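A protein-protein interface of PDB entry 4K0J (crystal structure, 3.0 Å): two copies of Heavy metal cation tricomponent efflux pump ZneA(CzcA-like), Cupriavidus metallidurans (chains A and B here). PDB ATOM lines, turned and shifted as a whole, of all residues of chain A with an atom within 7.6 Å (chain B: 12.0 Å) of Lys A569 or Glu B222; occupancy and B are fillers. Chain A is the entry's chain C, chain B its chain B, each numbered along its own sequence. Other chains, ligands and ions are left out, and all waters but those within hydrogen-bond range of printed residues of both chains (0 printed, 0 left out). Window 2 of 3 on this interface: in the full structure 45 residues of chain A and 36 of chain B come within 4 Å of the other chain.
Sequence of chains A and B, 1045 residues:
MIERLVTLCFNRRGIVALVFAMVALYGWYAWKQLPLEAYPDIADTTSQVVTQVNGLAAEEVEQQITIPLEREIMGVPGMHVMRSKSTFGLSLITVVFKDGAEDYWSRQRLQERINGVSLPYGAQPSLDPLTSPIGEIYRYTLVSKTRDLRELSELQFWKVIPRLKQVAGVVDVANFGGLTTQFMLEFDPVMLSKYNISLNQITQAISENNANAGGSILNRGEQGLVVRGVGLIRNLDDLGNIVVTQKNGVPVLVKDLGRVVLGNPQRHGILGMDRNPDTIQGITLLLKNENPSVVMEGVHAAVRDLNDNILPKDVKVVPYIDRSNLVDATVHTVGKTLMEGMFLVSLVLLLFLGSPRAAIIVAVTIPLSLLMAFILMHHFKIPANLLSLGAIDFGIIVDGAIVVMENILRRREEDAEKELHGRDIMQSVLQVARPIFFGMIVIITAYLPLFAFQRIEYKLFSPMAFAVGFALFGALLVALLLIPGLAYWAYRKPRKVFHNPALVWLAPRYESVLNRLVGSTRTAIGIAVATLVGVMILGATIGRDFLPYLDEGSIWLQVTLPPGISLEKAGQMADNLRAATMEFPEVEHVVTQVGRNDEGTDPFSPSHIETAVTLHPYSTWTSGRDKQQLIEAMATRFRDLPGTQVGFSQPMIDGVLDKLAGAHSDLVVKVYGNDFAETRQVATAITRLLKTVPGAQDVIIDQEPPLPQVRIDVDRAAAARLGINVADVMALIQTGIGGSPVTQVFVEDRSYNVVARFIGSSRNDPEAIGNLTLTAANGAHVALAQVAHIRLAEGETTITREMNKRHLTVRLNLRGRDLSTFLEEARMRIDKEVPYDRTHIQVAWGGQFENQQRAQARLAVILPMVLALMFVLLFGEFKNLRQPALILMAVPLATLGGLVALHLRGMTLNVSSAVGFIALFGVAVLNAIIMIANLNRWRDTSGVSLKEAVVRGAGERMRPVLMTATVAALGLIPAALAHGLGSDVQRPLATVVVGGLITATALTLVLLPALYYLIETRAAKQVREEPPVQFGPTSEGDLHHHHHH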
ATOM      1  N   ILE A 270     -23.632   1.207  16.121  1.00  0.00           N
ATOM      2  CA  ILE A 270     -24.064  -0.062  16.682  1.00  0.00           C
ATOM      3  C   ILE A 270     -25.009  -0.729  15.692  1.00  0.00           C
ATOM      4  O   ILE A 270     -25.792  -0.061  15.010  1.00  0.00           O
ATOM      5  CB  ILE A 270     -24.760   0.132  18.040  1.00  0.00           C
ATOM      6  CG1 ILE A 270     -23.867   0.943  18.978  1.00  0.00           C
ATOM      7  CG2 ILE A 270     -25.093  -1.205  18.676  1.00  0.00           C
ATOM      8  CD1 ILE A 270     -24.499   1.241  20.321  1.00  0.00           C
ATOM      9  N   LEU A 561     -33.715  10.089  13.698  1.00  0.00           N
ATOM     10  CA  LEU A 561     -33.827  10.208  15.141  1.00  0.00           C
ATOM     11  C   LEU A 561     -33.523  11.638  15.601  1.00  0.00           C
ATOM     12  O   LEU A 561     -32.980  12.434  14.833  1.00  0.00           O
ATOM     13  CB  LEU A 561     -32.879   9.207  15.803  1.00  0.00           C
ATOM     14  CG  LEU A 561     -33.486   7.918  16.357  1.00  0.00           C
ATOM     15  CD1 LEU A 561     -34.545   7.358  15.440  1.00  0.00           C
ATOM     16  CD2 LEU A 561     -32.400   6.899  16.596  1.00  0.00           C
ATOM     17  N   PRO A 562     -33.899  11.978  16.849  1.00  0.00           N
ATOM     18  CA  PRO A 562     -33.645  13.320  17.387  1.00  0.00           C
ATOM     19  C   PRO A 562     -32.172  13.730  17.325  1.00  0.00           C
ATOM     20  O   PRO A 562     -31.298  12.874  17.424  1.00  0.00           O
ATOM     21  CB  PRO A 562     -34.135  13.217  18.839  1.00  0.00           C
ATOM     22  CG  PRO A 562     -34.429  11.768  19.076  1.00  0.00           C
ATOM     23  CD  PRO A 562     -34.751  11.191  17.755  1.00  0.00           C
ATOM     24  N   PRO A 563     -31.904  15.035  17.151  1.00  0.00           N
ATOM     25  CA  PRO A 563     -30.563  15.600  16.964  1.00  0.00           C
ATOM     26  C   PRO A 563     -29.670  15.528  18.210  1.00  0.00           C
ATOM     27  O   PRO A 563     -30.143  15.704  19.330  1.00  0.00           O
ATOM     28  CB  PRO A 563     -30.861  17.061  16.621  1.00  0.00           C
ATOM     29  CG  PRO A 563     -32.147  17.343  17.314  1.00  0.00           C
ATOM     30  CD  PRO A 563     -32.939  16.086  17.154  1.00  0.00           C
ATOM     31  N   GLY A 564     -28.384  15.265  18.001  1.00  0.00           N
ATOM     32  CA  GLY A 564     -27.399  15.304  19.072  1.00  0.00           C
ATOM     33  C   GLY A 564     -27.382  14.101  19.993  1.00  0.00           C
ATOM     34  O   GLY A 564     -26.506  13.985  20.847  1.00  0.00           O
ATOM     35  N   ILE A 565     -28.357  13.214  19.812  1.00  0.00           N
ATOM     36  CA  ILE A 565     -28.523  12.011  20.620  1.00  0.00           C
ATOM     37  C   ILE A 565     -27.245  11.177  20.726  1.00  0.00           C
ATOM     38  O   ILE A 565     -26.570  10.928  19.729  1.00  0.00           O
ATOM     39  CB  ILE A 565     -29.669  11.149  20.052  1.00  0.00           C
ATOM     40  CG1 ILE A 565     -31.004  11.855  20.254  1.00  0.00           C
ATOM     41  CG2 ILE A 565     -29.715   9.793  20.713  1.00  0.00           C
ATOM     42  CD1 ILE A 565     -31.329  12.121  21.692  1.00  0.00           C
ATOM     43  N   SER A 566     -26.919  10.761  21.947  1.00  0.00           N
ATOM     44  CA  SER A 566     -25.766   9.911  22.213  1.00  0.00           C
ATOM     45  C   SER A 566     -25.935   8.574  21.523  1.00  0.00           C
ATOM     46  O   SER A 566     -27.022   8.239  21.072  1.00  0.00           O
ATOM     47  CB  SER A 566     -25.646   9.668  23.713  1.00  0.00           C
ATOM     48  OG  SER A 566     -26.694   8.827  24.161  1.00  0.00           O
ATOM     49  N   LEU A 567     -24.864   7.795  21.457  1.00  0.00           N
ATOM     50  CA  LEU A 567     -24.938   6.486  20.819  1.00  0.00           C
ATOM     51  C   LEU A 567     -25.693   5.456  21.676  1.00  0.00           C
ATOM     52  O   LEU A 567     -26.284   4.512  21.146  1.00  0.00           O
ATOM     53  CB  LEU A 567     -23.541   5.985  20.455  1.00  0.00           C
ATOM     54  CG  LEU A 567     -23.470   4.721  19.594  1.00  0.00           C
ATOM     55  CD1 LEU A 567     -24.140   4.940  18.249  1.00  0.00           C
ATOM     56  CD2 LEU A 567     -22.031   4.282  19.406  1.00  0.00           C
ATOM     57  N   GLU A 568     -25.687   5.642  22.995  1.00  0.00           N
ATOM     58  CA  GLU A 568     -26.435   4.753  23.876  1.00  0.00           C
ATOM     59  C   GLU A 568     -27.927   4.947  23.667  1.00  0.00           C
ATOM     60  O   GLU A 568     -28.663   3.986  23.425  1.00  0.00           O
ATOM     61  CB  GLU A 568     -26.074   4.973  25.351  1.00  0.00           C
ATOM     62  CG  GLU A 568     -26.652   3.902  26.294  1.00  0.00           C
ATOM     63  CD  GLU A 568     -26.332   4.150  27.768  1.00  0.00           C
ATOM     64  OE1 GLU A 568     -26.826   3.386  28.631  1.00  0.00           O
ATOM     65  OE2 GLU A 568     -25.589   5.109  28.069  1.00  0.00           O
ATOM     66  N   LYS A 569     -28.366   6.200  23.755  1.00  0.00           N
ATOM     67  CA  LYS A 569     -29.775   6.533  23.574  1.00  0.00           C
ATOM     68  C   LYS A 569     -30.265   6.111  22.193  1.00  0.00           C
ATOM     69  O   LYS A 569     -31.334   5.520  22.064  1.00  0.00           O
ATOM     70  CB  LYS A 569     -30.005   8.029  23.803  1.00  0.00           C
ATOM     71  CG  LYS A 569     -31.439   8.496  23.559  1.00  0.00           C
ATOM     72  CD  LYS A 569     -32.430   7.830  24.503  1.00  0.00           C
ATOM     73  CE  LYS A 569     -33.854   8.281  24.215  1.00  0.00           C
ATOM     74  NZ  LYS A 569     -34.843   7.596  25.097  1.00  0.00           N
ATOM     75  N   ALA A 570     -29.465   6.411  21.171  1.00  0.00           N
ATOM     76  CA  ALA A 570     -29.734   5.970  19.805  1.00  0.00           C
ATOM     77  C   ALA A 570     -29.956   4.478  19.787  1.00  0.00           C
ATOM     78  O   ALA A 570     -30.959   4.001  19.267  1.00  0.00           O
ATOM     79  CB  ALA A 570     -28.580   6.332  18.887  1.00  0.00           C
ATOM     80  N   GLY A 571     -29.016   3.748  20.375  1.00  0.00           N
ATOM     81  CA  GLY A 571     -29.113   2.302  20.477  1.00  0.00           C
ATOM     82  C   GLY A 571     -30.409   1.819  21.099  1.00  0.00           C
ATOM     83  O   GLY A 571     -31.013   0.861  20.622  1.00  0.00           O
ATOM     84  N   GLN A 572     -30.843   2.484  22.161  1.00  0.00           N
ATOM     85  CA  GLN A 572     -32.096   2.115  22.807  1.00  0.00           C
ATOM     86  C   GLN A 572     -33.297   2.378  21.899  1.00  0.00           C
ATOM     87  O   GLN A 572     -34.217   1.556  21.801  1.00  0.00           O
ATOM     88  CB  GLN A 572     -32.246   2.859  24.132  1.00  0.00           C
ATOM     89  CG  GLN A 572     -31.054   2.676  25.055  1.00  0.00           C
ATOM     90  CD  GLN A 572     -31.241   3.361  26.385  1.00  0.00           C
ATOM     91  OE1 GLN A 572     -32.226   3.123  27.083  1.00  0.00           O
ATOM     92  NE2 GLN A 572     -30.299   4.224  26.746  1.00  0.00           N
ATOM     93  N   MET A 573     -33.275   3.521  21.225  1.00  0.00           N
ATOM     94  CA  MET A 573     -34.353   3.879  20.323  1.00  0.00           C
ATOM     95  C   MET A 573     -34.469   2.858  19.205  1.00  0.00           C
ATOM     96  O   MET A 573     -35.569   2.460  18.820  1.00  0.00           O
ATOM     97  CB  MET A 573     -34.139   5.288  19.771  1.00  0.00           C
ATOM     98  CG  MET A 573     -34.248   6.362  20.844  1.00  0.00           C
ATOM     99  SD  MET A 573     -34.187   8.065  20.242  1.00  0.00           S
ATOM    100  CE  MET A 573     -35.882   8.327  19.736  1.00  0.00           C
ATOM    101  N   ALA A 574     -33.319   2.421  18.703  1.00  0.00           N
ATOM    102  CA  ALA A 574     -33.277   1.416  17.651  1.00  0.00           C
ATOM    103  C   ALA A 574     -33.791   0.077  18.170  1.00  0.00           C
ATOM    104  O   ALA A 574     -34.565  -0.595  17.489  1.00  0.00           O
ATOM    105  CB  ALA A 574     -31.876   1.279  17.111  1.00  0.00           C
ATOM    106  N   ASP A 575     -33.357  -0.296  19.374  1.00  0.00           N
ATOM    107  CA  ASP A 575     -33.868  -1.478  20.066  1.00  0.00           C
ATOM    108  C   ASP A 575     -35.391  -1.496  20.065  1.00  0.00           C
ATOM    109  O   ASP A 575     -36.020  -2.496  19.703  1.00  0.00           O
ATOM    110  CB  ASP A 575     -33.375  -1.504  21.513  1.00  0.00           C
ATOM    111  CG  ASP A 575     -31.922  -1.917  21.631  1.00  0.00           C
ATOM    112  OD1 ASP A 575     -31.454  -2.688  20.763  1.00  0.00           O
ATOM    113  OD2 ASP A 575     -31.253  -1.474  22.595  1.00  0.00           O
ATOM    114  N   ASN A 576     -35.977  -0.377  20.470  1.00  0.00           N
ATOM    115  CA  ASN A 576     -37.425  -0.265  20.497  1.00  0.00           C
ATOM    116  C   ASN A 576     -38.045  -0.365  19.108  1.00  0.00           C
ATOM    117  O   ASN A 576     -39.066  -1.038  18.924  1.00  0.00           O
ATOM    118  CB  ASN A 576     -37.845   1.036  21.175  1.00  0.00           C
ATOM    119  CG  ASN A 576     -37.503   1.057  22.644  1.00  0.00           C
ATOM    120  OD1 ASN A 576     -36.680   0.272  23.115  1.00  0.00           O
ATOM    121  ND2 ASN A 576     -38.136   1.960  23.382  1.00  0.00           N
ATOM    122  N   VAL A 594     -27.479   1.638  13.284  1.00  0.00           N
ATOM    123  CA  VAL A 594     -27.436   2.993  13.813  1.00  0.00           C
ATOM    124  C   VAL A 594     -25.999   3.489  13.794  1.00  0.00           C
ATOM    125  O   VAL A 594     -25.087   2.771  14.191  1.00  0.00           O
ATOM    126  CB  VAL A 594     -28.080   3.112  15.233  1.00  0.00           C
ATOM    127  CG1 VAL A 594     -28.154   1.758  15.919  1.00  0.00           C
ATOM    128  CG2 VAL A 594     -27.327   4.116  16.096  1.00  0.00           C
ATOM    129  N   PRO A 606     -25.287   8.880  15.207  1.00  0.00           N
ATOM    130  CA  PRO A 606     -26.192   7.947  15.892  1.00  0.00           C
ATOM    131  C   PRO A 606     -27.663   8.310  15.702  1.00  0.00           C
ATOM    132  O   PRO A 606     -28.543   7.464  15.879  1.00  0.00           O
ATOM    133  CB  PRO A 606     -25.799   8.097  17.361  1.00  0.00           C
ATOM    134  CG  PRO A 606     -24.377   8.506  17.320  1.00  0.00           C
ATOM    135  CD  PRO A 606     -24.243   9.391  16.117  1.00  0.00           C
ATOM    136  N   PRO A 642     -41.718   7.133  19.814  1.00  0.00           N
ATOM    137  CA  PRO A 642     -41.329   8.531  20.038  1.00  0.00           C
ATOM    138  C   PRO A 642     -39.968   8.885  19.440  1.00  0.00           C
ATOM    139  O   PRO A 642     -38.982   8.211  19.718  1.00  0.00           O
ATOM    140  CB  PRO A 642     -41.282   8.638  21.565  1.00  0.00           C
ATOM    141  CG  PRO A 642     -41.000   7.253  22.030  1.00  0.00           C
ATOM    142  CD  PRO A 642     -41.693   6.341  21.055  1.00  0.00           C
ATOM    143  N   ILE B 217     -16.395  12.529  20.771  1.00  0.00           N
ATOM    144  CA  ILE B 217     -17.682  12.799  21.394  1.00  0.00           C
ATOM    145  C   ILE B 217     -17.680  12.726  22.924  1.00  0.00           C
ATOM    146  O   ILE B 217     -17.323  11.705  23.507  1.00  0.00           O
ATOM    147  CB  ILE B 217     -18.769  11.855  20.858  1.00  0.00           C
ATOM    148  CG1 ILE B 217     -18.903  11.985  19.335  1.00  0.00           C
ATOM    149  CG2 ILE B 217     -20.081  12.136  21.550  1.00  0.00           C
ATOM    150  CD1 ILE B 217     -19.750  10.882  18.688  1.00  0.00           C
ATOM    151  N   LEU B 218     -18.080  13.825  23.562  1.00  0.00           N
ATOM    152  CA  LEU B 218     -18.339  13.839  25.000  1.00  0.00           C
ATOM    153  C   LEU B 218     -19.809  13.581  25.247  1.00  0.00           C
ATOM    154  O   LEU B 218     -20.668  14.290  24.718  1.00  0.00           O
ATOM    155  CB  LEU B 218     -17.983  15.185  25.623  1.00  0.00           C
ATOM    156  CG  LEU B 218     -16.499  15.512  25.756  1.00  0.00           C
ATOM    157  CD1 LEU B 218     -16.335  16.685  26.709  1.00  0.00           C
ATOM    158  CD2 LEU B 218     -15.711  14.291  26.229  1.00  0.00           C
ATOM    159  N   ASN B 219     -20.093  12.568  26.056  1.00  0.00           N
ATOM    160  CA  ASN B 219     -21.466  12.218  26.375  1.00  0.00           C
ATOM    161  C   ASN B 219     -21.914  12.867  27.669  1.00  0.00           C
ATOM    162  O   ASN B 219     -21.467  12.485  28.748  1.00  0.00           O
ATOM    163  CB  ASN B 219     -21.625  10.703  26.466  1.00  0.00           C
ATOM    164  CG  ASN B 219     -21.321  10.009  25.158  1.00  0.00           C
ATOM    165  OD1 ASN B 219     -22.089  10.101  24.203  1.00  0.00           O
ATOM    166  ND2 ASN B 219     -20.197   9.303  25.106  1.00  0.00           N
ATOM    167  N   ARG B 220     -22.792  13.858  27.554  1.00  0.00           N
ATOM    168  CA  ARG B 220     -23.342  14.527  28.723  1.00  0.00           C
ATOM    169  C   ARG B 220     -24.823  14.214  28.814  1.00  0.00           C
ATOM    170  O   ARG B 220     -25.665  15.070  28.550  1.00  0.00           O
ATOM    171  CB  ARG B 220     -23.125  16.038  28.635  1.00  0.00           C
ATOM    172  CG  ARG B 220     -22.831  16.711  29.970  1.00  0.00           C
ATOM    173  CD  ARG B 220     -22.577  18.207  29.795  1.00  0.00           C
ATOM    174  NE  ARG B 220     -22.040  18.822  31.007  1.00  0.00           N
ATOM    175  CZ  ARG B 220     -21.740  20.113  31.127  1.00  0.00           C
ATOM    176  NH1 ARG B 220     -21.919  20.946  30.106  1.00  0.00           N
ATOM    177  NH2 ARG B 220     -21.250  20.572  32.270  1.00  0.00           N
ATOM    178  N   GLY B 221     -25.132  12.974  29.180  1.00  0.00           N
ATOM    179  CA  GLY B 221     -26.507  12.521  29.288  1.00  0.00           C
ATOM    180  C   GLY B 221     -26.901  11.686  28.088  1.00  0.00           C
ATOM    181  O   GLY B 221     -26.226  10.712  27.749  1.00  0.00           O
ATOM    182  N   GLU B 222     -27.997  12.068  27.444  1.00  0.00           N
ATOM    183  CA  GLU B 222     -28.441  11.387  26.238  1.00  0.00           C
ATOM    184  C   GLU B 222     -27.923  12.105  25.002  1.00  0.00           C
ATOM    185  O   GLU B 222     -28.239  11.724  23.877  1.00  0.00           O
ATOM    186  CB  GLU B 222     -29.967  11.283  26.197  1.00  0.00           C
ATOM    187  CG  GLU B 222     -30.546  10.327  27.231  1.00  0.00           C
ATOM    188  CD  GLU B 222     -32.062  10.273  27.197  1.00  0.00           C
ATOM    189  OE1 GLU B 222     -32.661  10.917  26.306  1.00  0.00           O
ATOM    190  OE2 GLU B 222     -32.650   9.586  28.064  1.00  0.00           O
ATOM    191  N   GLN B 223     -27.122  13.145  25.214  1.00  0.00           N
ATOM    192  CA  GLN B 223     -26.519  13.870  24.100  1.00  0.00           C
ATOM    193  C   GLN B 223     -25.030  13.592  23.987  1.00  0.00           C
ATOM    194  O   GLN B 223     -24.395  13.153  24.941  1.00  0.00           O
ATOM    195  CB  GLN B 223     -26.774  15.376  24.204  1.00  0.00           C
ATOM    196  CG  GLN B 223     -28.075  15.833  23.548  1.00  0.00           C
ATOM    197  CD  GLN B 223     -27.992  17.253  23.015  1.00  0.00           C
ATOM    198  OE1 GLN B 223     -27.555  18.169  23.717  1.00  0.00           O
ATOM    199  NE2 GLN B 223     -28.399  17.440  21.763  1.00  0.00           N
ATOM    200  N   GLY B 224     -24.481  13.851  22.805  1.00  0.00           N
ATOM    201  CA  GLY B 224     -23.081  13.595  22.533  1.00  0.00           C
ATOM    202  C   GLY B 224     -22.470  14.695  21.691  1.00  0.00           C
ATOM    203  O   GLY B 224     -22.588  14.701  20.468  1.00  0.00           O
ATOM    204  N   LEU B 225     -21.802  15.625  22.359  1.00  0.00           N
ATOM    205  CA  LEU B 225     -21.278  16.823  21.715  1.00  0.00           C
ATOM    206  C   LEU B 225     -19.872  16.568  21.198  1.00  0.00           C
ATOM    207  O   LEU B 225     -19.038  16.016  21.914  1.00  0.00           O
ATOM    208  CB  LEU B 225     -21.213  17.959  22.727  1.00  0.00           C
ATOM    209  CG  LEU B 225     -22.461  18.669  23.246  1.00  0.00           C
ATOM    210  CD1 LEU B 225     -23.618  17.736  23.537  1.00  0.00           C
ATOM    211  CD2 LEU B 225     -22.069  19.414  24.508  1.00  0.00           C
ATOM    212  N   VAL B 226     -19.592  16.971  19.965  1.00  0.00           N
ATOM    213  CA  VAL B 226     -18.239  16.798  19.455  1.00  0.00           C
ATOM    214  C   VAL B 226     -17.373  17.913  20.013  1.00  0.00           C
ATOM    215  O   VAL B 226     -17.871  18.997  20.310  1.00  0.00           O
ATOM    216  CB  VAL B 226     -18.173  16.773  17.907  1.00  0.00           C
ATOM    217  CG1 VAL B 226     -18.937  15.588  17.370  1.00  0.00           C
ATOM    218  CG2 VAL B 226     -18.725  18.046  17.327  1.00  0.00           C
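The backbone NH of Lys A569 is in hydrogen-bond range of the side-chain hydroxyl of Ser A566, 3.1 Å away.
No position is printed for both chains.
O of Glu B222 sits at hydrogen-bond distance from N of Ser A566, 2.5 Å away. The backbone carbonyl oxygen of Pro A563 is in hydrogen-bond range of the side-chain amide nitrogen of Gln B223, at 3.5 Å. O of Gly A564 is in hydrogen-bond range of N of Gly B224 (2.8 Å).
Of the printed residues of chain B, Pro A563 touches Gln B223. Gly A564 touches two residues of chain B. Ser A566 touches just these residues of chain B: Asn B219 (3.6 Å), Glu B222 (2.5 Å) and Gln B223 (3.8 Å). No residue of chain B comes within 4 Å of Leu A567. No residue of chain B comes within 4 Å of Glu A568. Lys A569 touches just one residue of chain B: Glu B222 (3.6 Å). No residue of chain B comes within 4 Å of Gln A572. No residue of chain B comes within 4 Å of Met A573. Printed residues of chain A within 4 Å of Asn B219: Ser A566. No residue of chain A comes within 4 Å of Gly B221. Glu B222 touches three residues of chain A. Of the printed residues of chain A, Gln B223 touches Pro A563 (3.5 Å), Gly A564 (3.3 Å) and Ser A566 (3.8 Å). Of the printed residues of chain A, Gly B224 touches Gly A564 (2.8 Å).
Hydrophobic or aromatic side chains of chain A that line the printed part of chain B: Ile A565. Of the 10 printed residues of chain B, 4 touch a printed residue of chain A. Printed residues of chain B that touch a printed residue of chain A: Asn B219, Glu B222, Gln B223 and Gly B224. Along chain B the printed residues that touch a printed residue of chain A span positions 219 to 224.
Among the printed residues, pairs that only touch across the chains: Gly A564 with Gln B223, Ile A565 with Glu B222, Lys A569 with Glu B222, Ser A566 with Asn B219 and Ser A566 with Gln B223.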
